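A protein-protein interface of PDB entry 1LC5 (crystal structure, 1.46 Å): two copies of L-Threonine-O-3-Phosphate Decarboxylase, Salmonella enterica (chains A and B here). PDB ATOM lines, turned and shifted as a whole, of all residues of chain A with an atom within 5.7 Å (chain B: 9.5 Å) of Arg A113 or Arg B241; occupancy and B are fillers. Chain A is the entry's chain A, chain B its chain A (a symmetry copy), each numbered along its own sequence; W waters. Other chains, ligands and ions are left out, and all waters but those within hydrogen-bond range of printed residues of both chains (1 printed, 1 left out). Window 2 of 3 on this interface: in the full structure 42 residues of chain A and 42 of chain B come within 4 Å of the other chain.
Of the 11 printed residues of chain A, 4 touch a printed residue of chain B.
Printed residues of chain A that touch a printed residue of chain B: Phe A90, Glu A110, Arg A113 and Gln A117.
Hydrophobic or aromatic side chains of chain A that line the printed part of chain B: Phe A90.
Printed residues of chain B that touch a printed residue of chain A: Arg B241, Gln B242, Met B244 and Pro B245.
Hydrophobic or aromatic side chains of chain B within 4 Å of the printed part of chain A: Met B244 and Pro B245.
Water W1 lies within hydrogen-bond range of the backbone carbonyl oxygen of Gln B242 (2.7 Å) and the side-chain amide nitrogen of Gln A117 (2.7 Å).
NH1 of Arg A113 lies within salt-bridge range of OE1 of Glu A110, at 2.9 Å.
OG of Ser B94 sits close to NE2 of Gln B242 (3.3 Å).
The guanidinium group (NH2) of Arg A113 lies within hydrogen-bond range of the backbone carbonyl oxygen (O) of Arg B241 (2.9 Å).
Among the printed residues, merely in contact across the chains: Phe A90 with Met B244, Glu A110 with Pro B245, Arg A113 with Pro B245, Gln A117 with Arg B241 and Gln A117 with Gln B242.
No position is printed for both chains.
Of the 6 pairs that touch across the chains among the printed residues, none has its exchanged pair printed and touching as well.
Arg B241 touches just these residues of chain A: Arg A113 (2.9 Å) and Gln A117 (3.5 Å).
Of the printed residues of chain B, Gln A117 touches Arg B241 and Gln B242.
Of the printed residues of chain A, Gln B242 touches Gln A117.
Printed residues of chain A within 4 Å of Met B244: Phe A90.
Ser A118 touches none of the printed residues of chain B.
The nearest residue of chain B that does not touch Arg A113 is Gln B242 (5.0 Å).
The nearest printed residue of chain A that does not touch Arg B241 is Phe A90 (6.5 Å).
The nearest printed residue of chain B that does not touch Gln A117 is Gln B243 (5.6 Å).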
ATOM      1  N   PHE A  90      11.971  27.763  25.934  1.00  0.00           N
ATOM      2  CA  PHE A  90      13.124  27.495  25.086  1.00  0.00           C
ATOM      3  C   PHE A  90      14.338  28.258  25.575  1.00  0.00           C
ATOM      4  O   PHE A  90      15.446  27.710  25.565  1.00  0.00           O
ATOM      5  CB  PHE A  90      12.796  27.819  23.618  1.00  0.00           C
ATOM      6  CG  PHE A  90      11.961  26.768  22.946  1.00  0.00           C
ATOM      7  CD1 PHE A  90      10.581  26.775  23.078  1.00  0.00           C
ATOM      8  CD2 PHE A  90      12.557  25.738  22.222  1.00  0.00           C
ATOM      9  CE1 PHE A  90       9.806  25.762  22.500  1.00  0.00           C
ATOM     10  CE2 PHE A  90      11.799  24.727  21.645  1.00  0.00           C
ATOM     11  CZ  PHE A  90      10.425  24.735  21.773  1.00  0.00           C
ATOM     12  N   ALA A 109       4.020  19.598  26.042  1.00  0.00           N
ATOM     13  CA  ALA A 109       5.011  19.002  25.153  1.00  0.00           C
ATOM     14  C   ALA A 109       6.268  19.793  24.890  1.00  0.00           C
ATOM     15  O   ALA A 109       7.324  19.212  24.581  1.00  0.00           O
ATOM     16  CB  ALA A 109       4.351  18.649  23.809  1.00  0.00           C
ATOM     17  N   GLU A 110       6.174  21.111  25.018  1.00  0.00           N
ATOM     18  CA  GLU A 110       7.341  21.906  24.671  1.00  0.00           C
ATOM     19  C   GLU A 110       8.546  21.785  25.586  1.00  0.00           C
ATOM     20  O   GLU A 110       9.637  22.107  25.143  1.00  0.00           O
ATOM     21  CB  GLU A 110       6.947  23.370  24.462  1.00  0.00           C
ATOM     22  CG  GLU A 110       5.867  23.556  23.351  1.00  0.00           C
ATOM     23  CD  GLU A 110       6.274  22.991  21.991  1.00  0.00           C
ATOM     24  OE1 GLU A 110       7.470  23.051  21.652  1.00  0.00           O
ATOM     25  OE2 GLU A 110       5.424  22.478  21.227  1.00  0.00           O
ATOM     26  N   TYR A 111       8.396  21.302  26.819  1.00  0.00           N
ATOM     27  CA  TYR A 111       9.593  21.140  27.666  1.00  0.00           C
ATOM     28  C   TYR A 111      10.514  20.126  26.998  1.00  0.00           C
ATOM     29  O   TYR A 111      11.710  20.386  26.844  1.00  0.00           O
ATOM     30  CB  TYR A 111       9.260  20.612  29.065  1.00  0.00           C
ATOM     31  CG  TYR A 111       8.133  21.293  29.837  1.00  0.00           C
ATOM     32  CD1 TYR A 111       7.867  22.661  29.762  1.00  0.00           C
ATOM     33  CD2 TYR A 111       7.314  20.511  30.649  1.00  0.00           C
ATOM     34  CE1 TYR A 111       6.810  23.232  30.475  1.00  0.00           C
ATOM     35  CE2 TYR A 111       6.250  21.064  31.367  1.00  0.00           C
ATOM     36  CZ  TYR A 111       5.999  22.417  31.272  1.00  0.00           C
ATOM     37  OH  TYR A 111       4.909  22.944  31.938  1.00  0.00           O
ATOM     38  N   GLY A 112       9.961  18.982  26.609  1.00  0.00           N
ATOM     39  CA  GLY A 112      10.739  17.936  25.970  1.00  0.00           C
ATOM     40  C   GLY A 112      11.298  18.391  24.649  1.00  0.00           C
ATOM     41  O   GLY A 112      12.441  18.063  24.312  1.00  0.00           O
ATOM     42  N   ARG A 113      10.530  19.161  23.882  1.00  0.00           N
ATOM     43  CA  ARG A 113      11.043  19.626  22.590  1.00  0.00           C
ATOM     44  C   ARG A 113      12.215  20.570  22.777  1.00  0.00           C
ATOM     45  O   ARG A 113      13.235  20.459  22.075  1.00  0.00           O
ATOM     46  CB  ARG A 113       9.939  20.300  21.772  1.00  0.00           C
ATOM     47  CG  ARG A 113       8.805  19.307  21.426  1.00  0.00           C
ATOM     48  CD  ARG A 113       7.812  19.893  20.401  1.00  0.00           C
ATOM     49  NE  ARG A 113       8.474  20.038  19.093  1.00  0.00           N
ATOM     50  CZ  ARG A 113       8.915  21.185  18.569  1.00  0.00           C
ATOM     51  NH1 ARG A 113       8.764  22.351  19.196  1.00  0.00           N
ATOM     52  NH2 ARG A 113       9.581  21.131  17.417  1.00  0.00           N
ATOM     53  N   ALA A 114      12.110  21.477  23.737  1.00  0.00           N
ATOM     54  CA  ALA A 114      13.198  22.410  23.999  1.00  0.00           C
ATOM     55  C   ALA A 114      14.444  21.672  24.493  1.00  0.00           C
ATOM     56  O   ALA A 114      15.578  21.973  24.076  1.00  0.00           O
ATOM     57  CB  ALA A 114      12.734  23.456  25.025  1.00  0.00           C
ATOM     58  N   LEU A 115      14.262  20.713  25.383  1.00  0.00           N
ATOM     59  CA  LEU A 115      15.399  19.959  25.914  1.00  0.00           C
ATOM     60  C   LEU A 115      16.055  19.139  24.830  1.00  0.00           C
ATOM     61  O   LEU A 115      17.287  19.065  24.798  1.00  0.00           O
ATOM     62  CB  LEU A 115      14.918  19.073  27.052  1.00  0.00           C
ATOM     63  CG  LEU A 115      14.524  19.847  28.313  1.00  0.00           C
ATOM     64  CD1 LEU A 115      13.779  18.950  29.267  1.00  0.00           C
ATOM     65  CD2 LEU A 115      15.767  20.373  29.009  1.00  0.00           C
ATOM     66  N   ALA A 116      15.273  18.525  23.946  1.00  0.00           N
ATOM     67  CA  ALA A 116      15.846  17.725  22.865  1.00  0.00           C
ATOM     68  C   ALA A 116      16.652  18.618  21.924  1.00  0.00           C
ATOM     69  O   ALA A 116      17.734  18.230  21.465  1.00  0.00           O
ATOM     70  CB  ALA A 116      14.736  16.999  22.090  1.00  0.00           C
ATOM     71  N   GLN A 117      16.144  19.810  21.630  1.00  0.00           N
ATOM     72  CA  GLN A 117      16.854  20.725  20.741  1.00  0.00           C
ATOM     73  C   GLN A 117      18.197  21.143  21.331  1.00  0.00           C
ATOM     74  O   GLN A 117      19.144  21.431  20.593  1.00  0.00           O
ATOM     75  CB  GLN A 117      15.968  21.939  20.422  1.00  0.00           C
ATOM     76  CG  GLN A 117      14.859  21.520  19.454  1.00  0.00           C
ATOM     77  CD  GLN A 117      13.902  22.632  19.086  1.00  0.00           C
ATOM     78  OE1 GLN A 117      12.868  22.375  18.457  1.00  0.00           O
ATOM     79  NE2 GLN A 117      14.227  23.858  19.459  1.00  0.00           N
ATOM     80  N   SER A 118      18.297  21.137  22.658  1.00  0.00           N
ATOM     81  CA  SER A 118      19.541  21.506  23.323  1.00  0.00           C
ATOM     82  C   SER A 118      20.444  20.293  23.580  1.00  0.00           C
ATOM     83  O   SER A 118      21.496  20.432  24.204  1.00  0.00           O
ATOM     84  CB  SER A 118      19.238  22.242  24.640  1.00  0.00           C
ATOM     85  OG  SER A 118      18.474  21.438  25.523  1.00  0.00           O
ATOM     86  N   ALA B  59      -1.042  27.882  14.309  1.00  0.00           N
ATOM     87  CA  ALA B  59       0.321  27.387  14.457  1.00  0.00           C
ATOM     88  C   ALA B  59       1.023  27.097  13.130  1.00  0.00           C
ATOM     89  O   ALA B  59       2.244  27.145  13.050  1.00  0.00           O
ATOM     90  CB  ALA B  59       0.328  26.130  15.346  1.00  0.00           C
ATOM     91  N   ASP B  60       0.227  26.829  12.099  1.00  0.00           N
ATOM     92  CA  ASP B  60       0.770  26.549  10.768  1.00  0.00           C
ATOM     93  C   ASP B  60       0.846  27.784   9.881  1.00  0.00           C
ATOM     94  O   ASP B  60       1.465  27.728   8.807  1.00  0.00           O
ATOM     95  CB  ASP B  60      -0.070  25.483  10.069  1.00  0.00           C
ATOM     96  CG  ASP B  60      -0.067  24.165  10.808  1.00  0.00           C
ATOM     97  OD1 ASP B  60       1.023  23.695  11.167  1.00  0.00           O
ATOM     98  OD2 ASP B  60      -1.159  23.608  11.037  1.00  0.00           O
ATOM     99  N   LEU B  80       8.601  30.186   5.272  1.00  0.00           N
ATOM    100  CA  LEU B  80       8.388  30.120   6.707  1.00  0.00           C
ATOM    101  C   LEU B  80       8.566  31.527   7.280  1.00  0.00           C
ATOM    102  O   LEU B  80       9.684  32.062   7.310  1.00  0.00           O
ATOM    103  CB  LEU B  80       9.374  29.145   7.382  1.00  0.00           C
ATOM    104  CG  LEU B  80       9.259  29.133   8.905  1.00  0.00           C
ATOM    105  CD1 LEU B  80       7.871  28.697   9.346  1.00  0.00           C
ATOM    106  CD2 LEU B  80      10.311  28.181   9.486  1.00  0.00           C
ATOM    107  N   THR B  91      16.665  30.728  12.730  1.00  0.00           N
ATOM    108  CA  THR B  91      16.080  29.486  12.262  1.00  0.00           C
ATOM    109  C   THR B  91      16.928  28.827  11.182  1.00  0.00           C
ATOM    110  O   THR B  91      17.186  27.632  11.243  1.00  0.00           O
ATOM    111  CB  THR B  91      14.669  29.762  11.729  1.00  0.00           C
ATOM    112  OG1 THR B  91      13.841  30.145  12.846  1.00  0.00           O
ATOM    113  CG2 THR B  91      14.087  28.537  11.009  1.00  0.00           C
ATOM    114  N   SER B  94      20.165  27.363  12.777  1.00  0.00           N
ATOM    115  CA  SER B  94      19.935  26.175  13.604  1.00  0.00           C
ATOM    116  C   SER B  94      19.423  24.999  12.787  1.00  0.00           C
ATOM    117  O   SER B  94      19.763  23.852  13.095  1.00  0.00           O
ATOM    118  CB  SER B  94      18.939  26.499  14.723  1.00  0.00           C
ATOM    119  OG  SER B  94      17.706  26.918  14.183  1.00  0.00           O
ATOM    120  N   GLY B  95      18.617  25.255  11.752  1.00  0.00           N
ATOM    121  CA  GLY B  95      18.077  24.190  10.928  1.00  0.00           C
ATOM    122  C   GLY B  95      19.103  23.612   9.993  1.00  0.00           C
ATOM    123  O   GLY B  95      18.983  22.442   9.606  1.00  0.00           O
ATOM    124  N   ASP B 233      12.097  20.494  -0.136  1.00  0.00           N
ATOM    125  CA  ASP B 233      10.989  20.069   0.686  1.00  0.00           C
ATOM    126  C   ASP B 233      11.390  19.604   2.081  1.00  0.00           C
ATOM    127  O   ASP B 233      10.840  20.068   3.088  1.00  0.00           O
ATOM    128  CB  ASP B 233      10.191  18.938   0.006  1.00  0.00           C
ATOM    129  CG  ASP B 233       9.569  19.361  -1.305  1.00  0.00           C
ATOM    130  OD1 ASP B 233       9.134  20.526  -1.420  1.00  0.00           O
ATOM    131  OD2 ASP B 233       9.487  18.505  -2.226  1.00  0.00           O
ATOM    132  N   ALA B 234      12.348  18.683   2.156  1.00  0.00           N
ATOM    133  CA  ALA B 234      12.768  18.161   3.434  1.00  0.00           C
ATOM    134  C   ALA B 234      13.386  19.199   4.353  1.00  0.00           C
ATOM    135  O   ALA B 234      13.110  19.220   5.560  1.00  0.00           O
ATOM    136  CB  ALA B 234      13.757  17.010   3.240  1.00  0.00           C
ATOM    137  N   ALA B 235      14.210  20.077   3.786  1.00  0.00           N
ATOM    138  CA  ALA B 235      14.887  21.056   4.619  1.00  0.00           C
ATOM    139  C   ALA B 235      13.879  22.050   5.176  1.00  0.00           C
ATOM    140  O   ALA B 235      13.962  22.391   6.344  1.00  0.00           O
ATOM    141  CB  ALA B 235      15.997  21.756   3.843  1.00  0.00           C
ATOM    142  N   MET B 236      12.928  22.513   4.361  1.00  0.00           N
ATOM    143  CA  MET B 236      11.920  23.443   4.887  1.00  0.00           C
ATOM    144  C   MET B 236      11.040  22.783   5.938  1.00  0.00           C
ATOM    145  O   MET B 236      10.675  23.404   6.944  1.00  0.00           O
ATOM    146  CB  MET B 236      11.083  24.024   3.755  1.00  0.00           C
ATOM    147  CG  MET B 236      11.794  25.160   3.040  1.00  0.00           C
ATOM    148  SD  MET B 236      12.228  26.574   4.101  1.00  0.00           S
ATOM    149  CE  MET B 236      10.624  27.159   4.585  1.00  0.00           C
ATOM    150  N   ALA B 237      10.722  21.501   5.757  1.00  0.00           N
ATOM    151  CA  ALA B 237       9.945  20.816   6.781  1.00  0.00           C
ATOM    152  C   ALA B 237      10.716  20.809   8.107  1.00  0.00           C
ATOM    153  O   ALA B 237      10.148  21.011   9.198  1.00  0.00           O
ATOM    154  CB  ALA B 237       9.646  19.378   6.346  1.00  0.00           C
ATOM    155  N   ARG B 238      12.022  20.595   8.017  1.00  0.00           N
ATOM    156  CA  ARG B 238      12.838  20.617   9.219  1.00  0.00           C
ATOM    157  C   ARG B 238      12.845  22.035   9.837  1.00  0.00           C
ATOM    158  O   ARG B 238      12.806  22.198  11.075  1.00  0.00           O
ATOM    159  CB  ARG B 238      14.249  20.133   8.874  1.00  0.00           C
ATOM    160  CG  ARG B 238      15.169  20.038  10.080  1.00  0.00           C
ATOM    161  CD  ARG B 238      16.466  19.322   9.714  1.00  0.00           C
ATOM    162  NE  ARG B 238      17.329  20.151   8.895  1.00  0.00           N
ATOM    163  CZ  ARG B 238      17.622  19.951   7.620  1.00  0.00           C
ATOM    164  NH1 ARG B 238      18.436  20.792   7.010  1.00  0.00           N
ATOM    165  NH2 ARG B 238      17.110  18.930   6.932  1.00  0.00           N
ATOM    166  N   MET B 239      12.908  23.067   9.001  1.00  0.00           N
ATOM    167  CA  MET B 239      12.877  24.441   9.517  1.00  0.00           C
ATOM    168  C   MET B 239      11.596  24.714  10.306  1.00  0.00           C
ATOM    169  O   MET B 239      11.642  25.416  11.342  1.00  0.00           O
ATOM    170  CB  MET B 239      12.961  25.477   8.389  1.00  0.00           C
ATOM    171  CG  MET B 239      14.279  25.476   7.618  1.00  0.00           C
ATOM    172  SD  MET B 239      15.683  25.974   8.667  1.00  0.00           S
ATOM    173  CE  MET B 239      17.004  25.363   7.664  1.00  0.00           C
ATOM    174  N   ARG B 240      10.462  24.198   9.842  1.00  0.00           N
ATOM    175  CA  ARG B 240       9.223  24.422  10.567  1.00  0.00           C
ATOM    176  C   ARG B 240       9.264  23.790  11.950  1.00  0.00           C
ATOM    177  O   ARG B 240       8.640  24.287  12.877  1.00  0.00           O
ATOM    178  CB  ARG B 240       8.044  23.878   9.772  1.00  0.00           C
ATOM    179  CG  ARG B 240       7.822  24.625   8.458  1.00  0.00           C
ATOM    180  CD  ARG B 240       6.497  24.248   7.772  1.00  0.00           C
ATOM    181  NE  ARG B 240       6.650  24.631   6.370  1.00  0.00           N
ATOM    182  CZ  ARG B 240       6.467  25.846   5.882  1.00  0.00           C
ATOM    183  NH1 ARG B 240       6.062  26.841   6.663  1.00  0.00           N
ATOM    184  NH2 ARG B 240       6.804  26.088   4.619  1.00  0.00           N
ATOM    185  N   ARG B 241       9.993  22.680  12.100  1.00  0.00           N
ATOM    186  CA  ARG B 241      10.113  22.037  13.414  1.00  0.00           C
ATOM    187  C   ARG B 241      11.124  22.763  14.296  1.00  0.00           C
ATOM    188  O   ARG B 241      10.965  22.845  15.513  1.00  0.00           O
ATOM    189  CB  ARG B 241      10.526  20.572  13.252  1.00  0.00           C
ATOM    190  CG  ARG B 241       9.510  19.718  12.494  1.00  0.00           C
ATOM    191  CD  ARG B 241       9.928  18.227  12.554  1.00  0.00           C
ATOM    192  NE  ARG B 241      11.124  17.906  11.767  1.00  0.00           N
ATOM    193  CZ  ARG B 241      11.097  17.557  10.479  1.00  0.00           C
ATOM    194  NH1 ARG B 241       9.948  17.479   9.823  1.00  0.00           N
ATOM    195  NH2 ARG B 241      12.221  17.292   9.844  1.00  0.00           N
ATOM    196  N   GLN B 242      12.156  23.338  13.689  1.00  0.00           N
ATOM    197  CA  GLN B 242      13.190  24.043  14.435  1.00  0.00           C
ATOM    198  C   GLN B 242      12.710  25.361  15.044  1.00  0.00           C
ATOM    199  O   GLN B 242      13.109  25.759  16.149  1.00  0.00           O
ATOM    200  CB  GLN B 242      14.372  24.309  13.496  1.00  0.00           C
ATOM    201  CG  GLN B 242      15.541  25.020  14.127  1.00  0.00           C
ATOM    202  CD  GLN B 242      16.109  24.288  15.324  1.00  0.00           C
ATOM    203  OE1 GLN B 242      16.409  23.094  15.252  1.00  0.00           O
ATOM    204  NE2 GLN B 242      16.271  25.006  16.436  1.00  0.00           N
ATOM    205  N   GLN B 243      11.864  26.068  14.319  1.00  0.00           N
ATOM    206  CA  GLN B 243      11.394  27.348  14.822  1.00  0.00           C
ATOM    207  C   GLN B 243      10.349  27.157  15.923  1.00  0.00           C
ATOM    208  O   GLN B 243       9.452  26.303  15.840  1.00  0.00           O
ATOM    209  CB  GLN B 243      10.817  28.156  13.655  1.00  0.00           C
ATOM    210  CG  GLN B 243      10.539  29.644  13.993  1.00  0.00           C
ATOM    211  CD  GLN B 243      10.346  30.449  12.727  1.00  0.00           C
ATOM    212  OE1 GLN B 243      11.309  30.795  12.025  1.00  0.00           O
ATOM    213  NE2 GLN B 243       9.095  30.750  12.425  1.00  0.00           N
ATOM    214  N   MET B 244      10.440  27.977  16.956  1.00  0.00           N
ATOM    215  CA  MET B 244       9.496  27.869  18.069  1.00  0.00           C
ATOM    216  C   MET B 244       8.005  28.012  17.694  1.00  0.00           C
ATOM    217  O   MET B 244       7.661  28.852  16.853  1.00  0.00           O
ATOM    218  CB  MET B 244       9.824  28.957  19.067  1.00  0.00           C
ATOM    219  CG  MET B 244       8.941  29.006  20.246  1.00  0.00           C
ATOM    220  SD  MET B 244       9.491  30.401  21.194  1.00  0.00           S
ATOM    221  CE  MET B 244      11.211  30.193  21.011  1.00  0.00           C
ATOM    222  N   PRO B 245       7.103  27.240  18.336  1.00  0.00           N
ATOM    223  CA  PRO B 245       5.682  27.365  18.019  1.00  0.00           C
ATOM    224  C   PRO B 245       5.140  28.783  18.335  1.00  0.00           C
ATOM    225  O   PRO B 245       5.577  29.426  19.307  1.00  0.00           O
ATOM    226  CB  PRO B 245       5.010  26.338  18.930  1.00  0.00           C
ATOM    227  CG  PRO B 245       6.121  25.300  19.168  1.00  0.00           C
ATOM    228  CD  PRO B 245       7.378  26.114  19.260  1.00  0.00           C
ATOM    229  N   TRP B 246       4.207  29.253  17.488  1.00  0.00           N
ATOM    230  CA  TRP B 246       3.499  30.534  17.660  1.00  0.00           C
ATOM    231  C   TRP B 246       4.436  31.705  17.768  1.00  0.00           C
ATOM    232  O   TRP B 246       4.142  32.680  18.465  1.00  0.00           O
ATOM    233  CB  TRP B 246       2.614  30.510  18.934  1.00  0.00           C
ATOM    234  CG  TRP B 246       1.638  29.349  19.081  1.00  0.00           C
ATOM    235  CD1 TRP B 246       0.551  29.056  18.287  1.00  0.00           C
ATOM    236  CD2 TRP B 246       1.615  28.412  20.156  1.00  0.00           C
ATOM    237  NE1 TRP B 246      -0.146  27.984  18.821  1.00  0.00           N
ATOM    238  CE2 TRP B 246       0.488  27.576  19.966  1.00  0.00           C
ATOM    239  CE3 TRP B 246       2.440  28.202  21.275  1.00  0.00           C
ATOM    240  CZ2 TRP B 246       0.172  26.543  20.856  1.00  0.00           C
ATOM    241  CZ3 TRP B 246       2.128  27.178  22.151  1.00  0.00           C
ATOM    242  CH2 TRP B 246       1.000  26.362  21.936  1.00  0.00           C
HETATM  243  O   HOH W   1      12.730  26.047  18.812  1.00  0.00           O
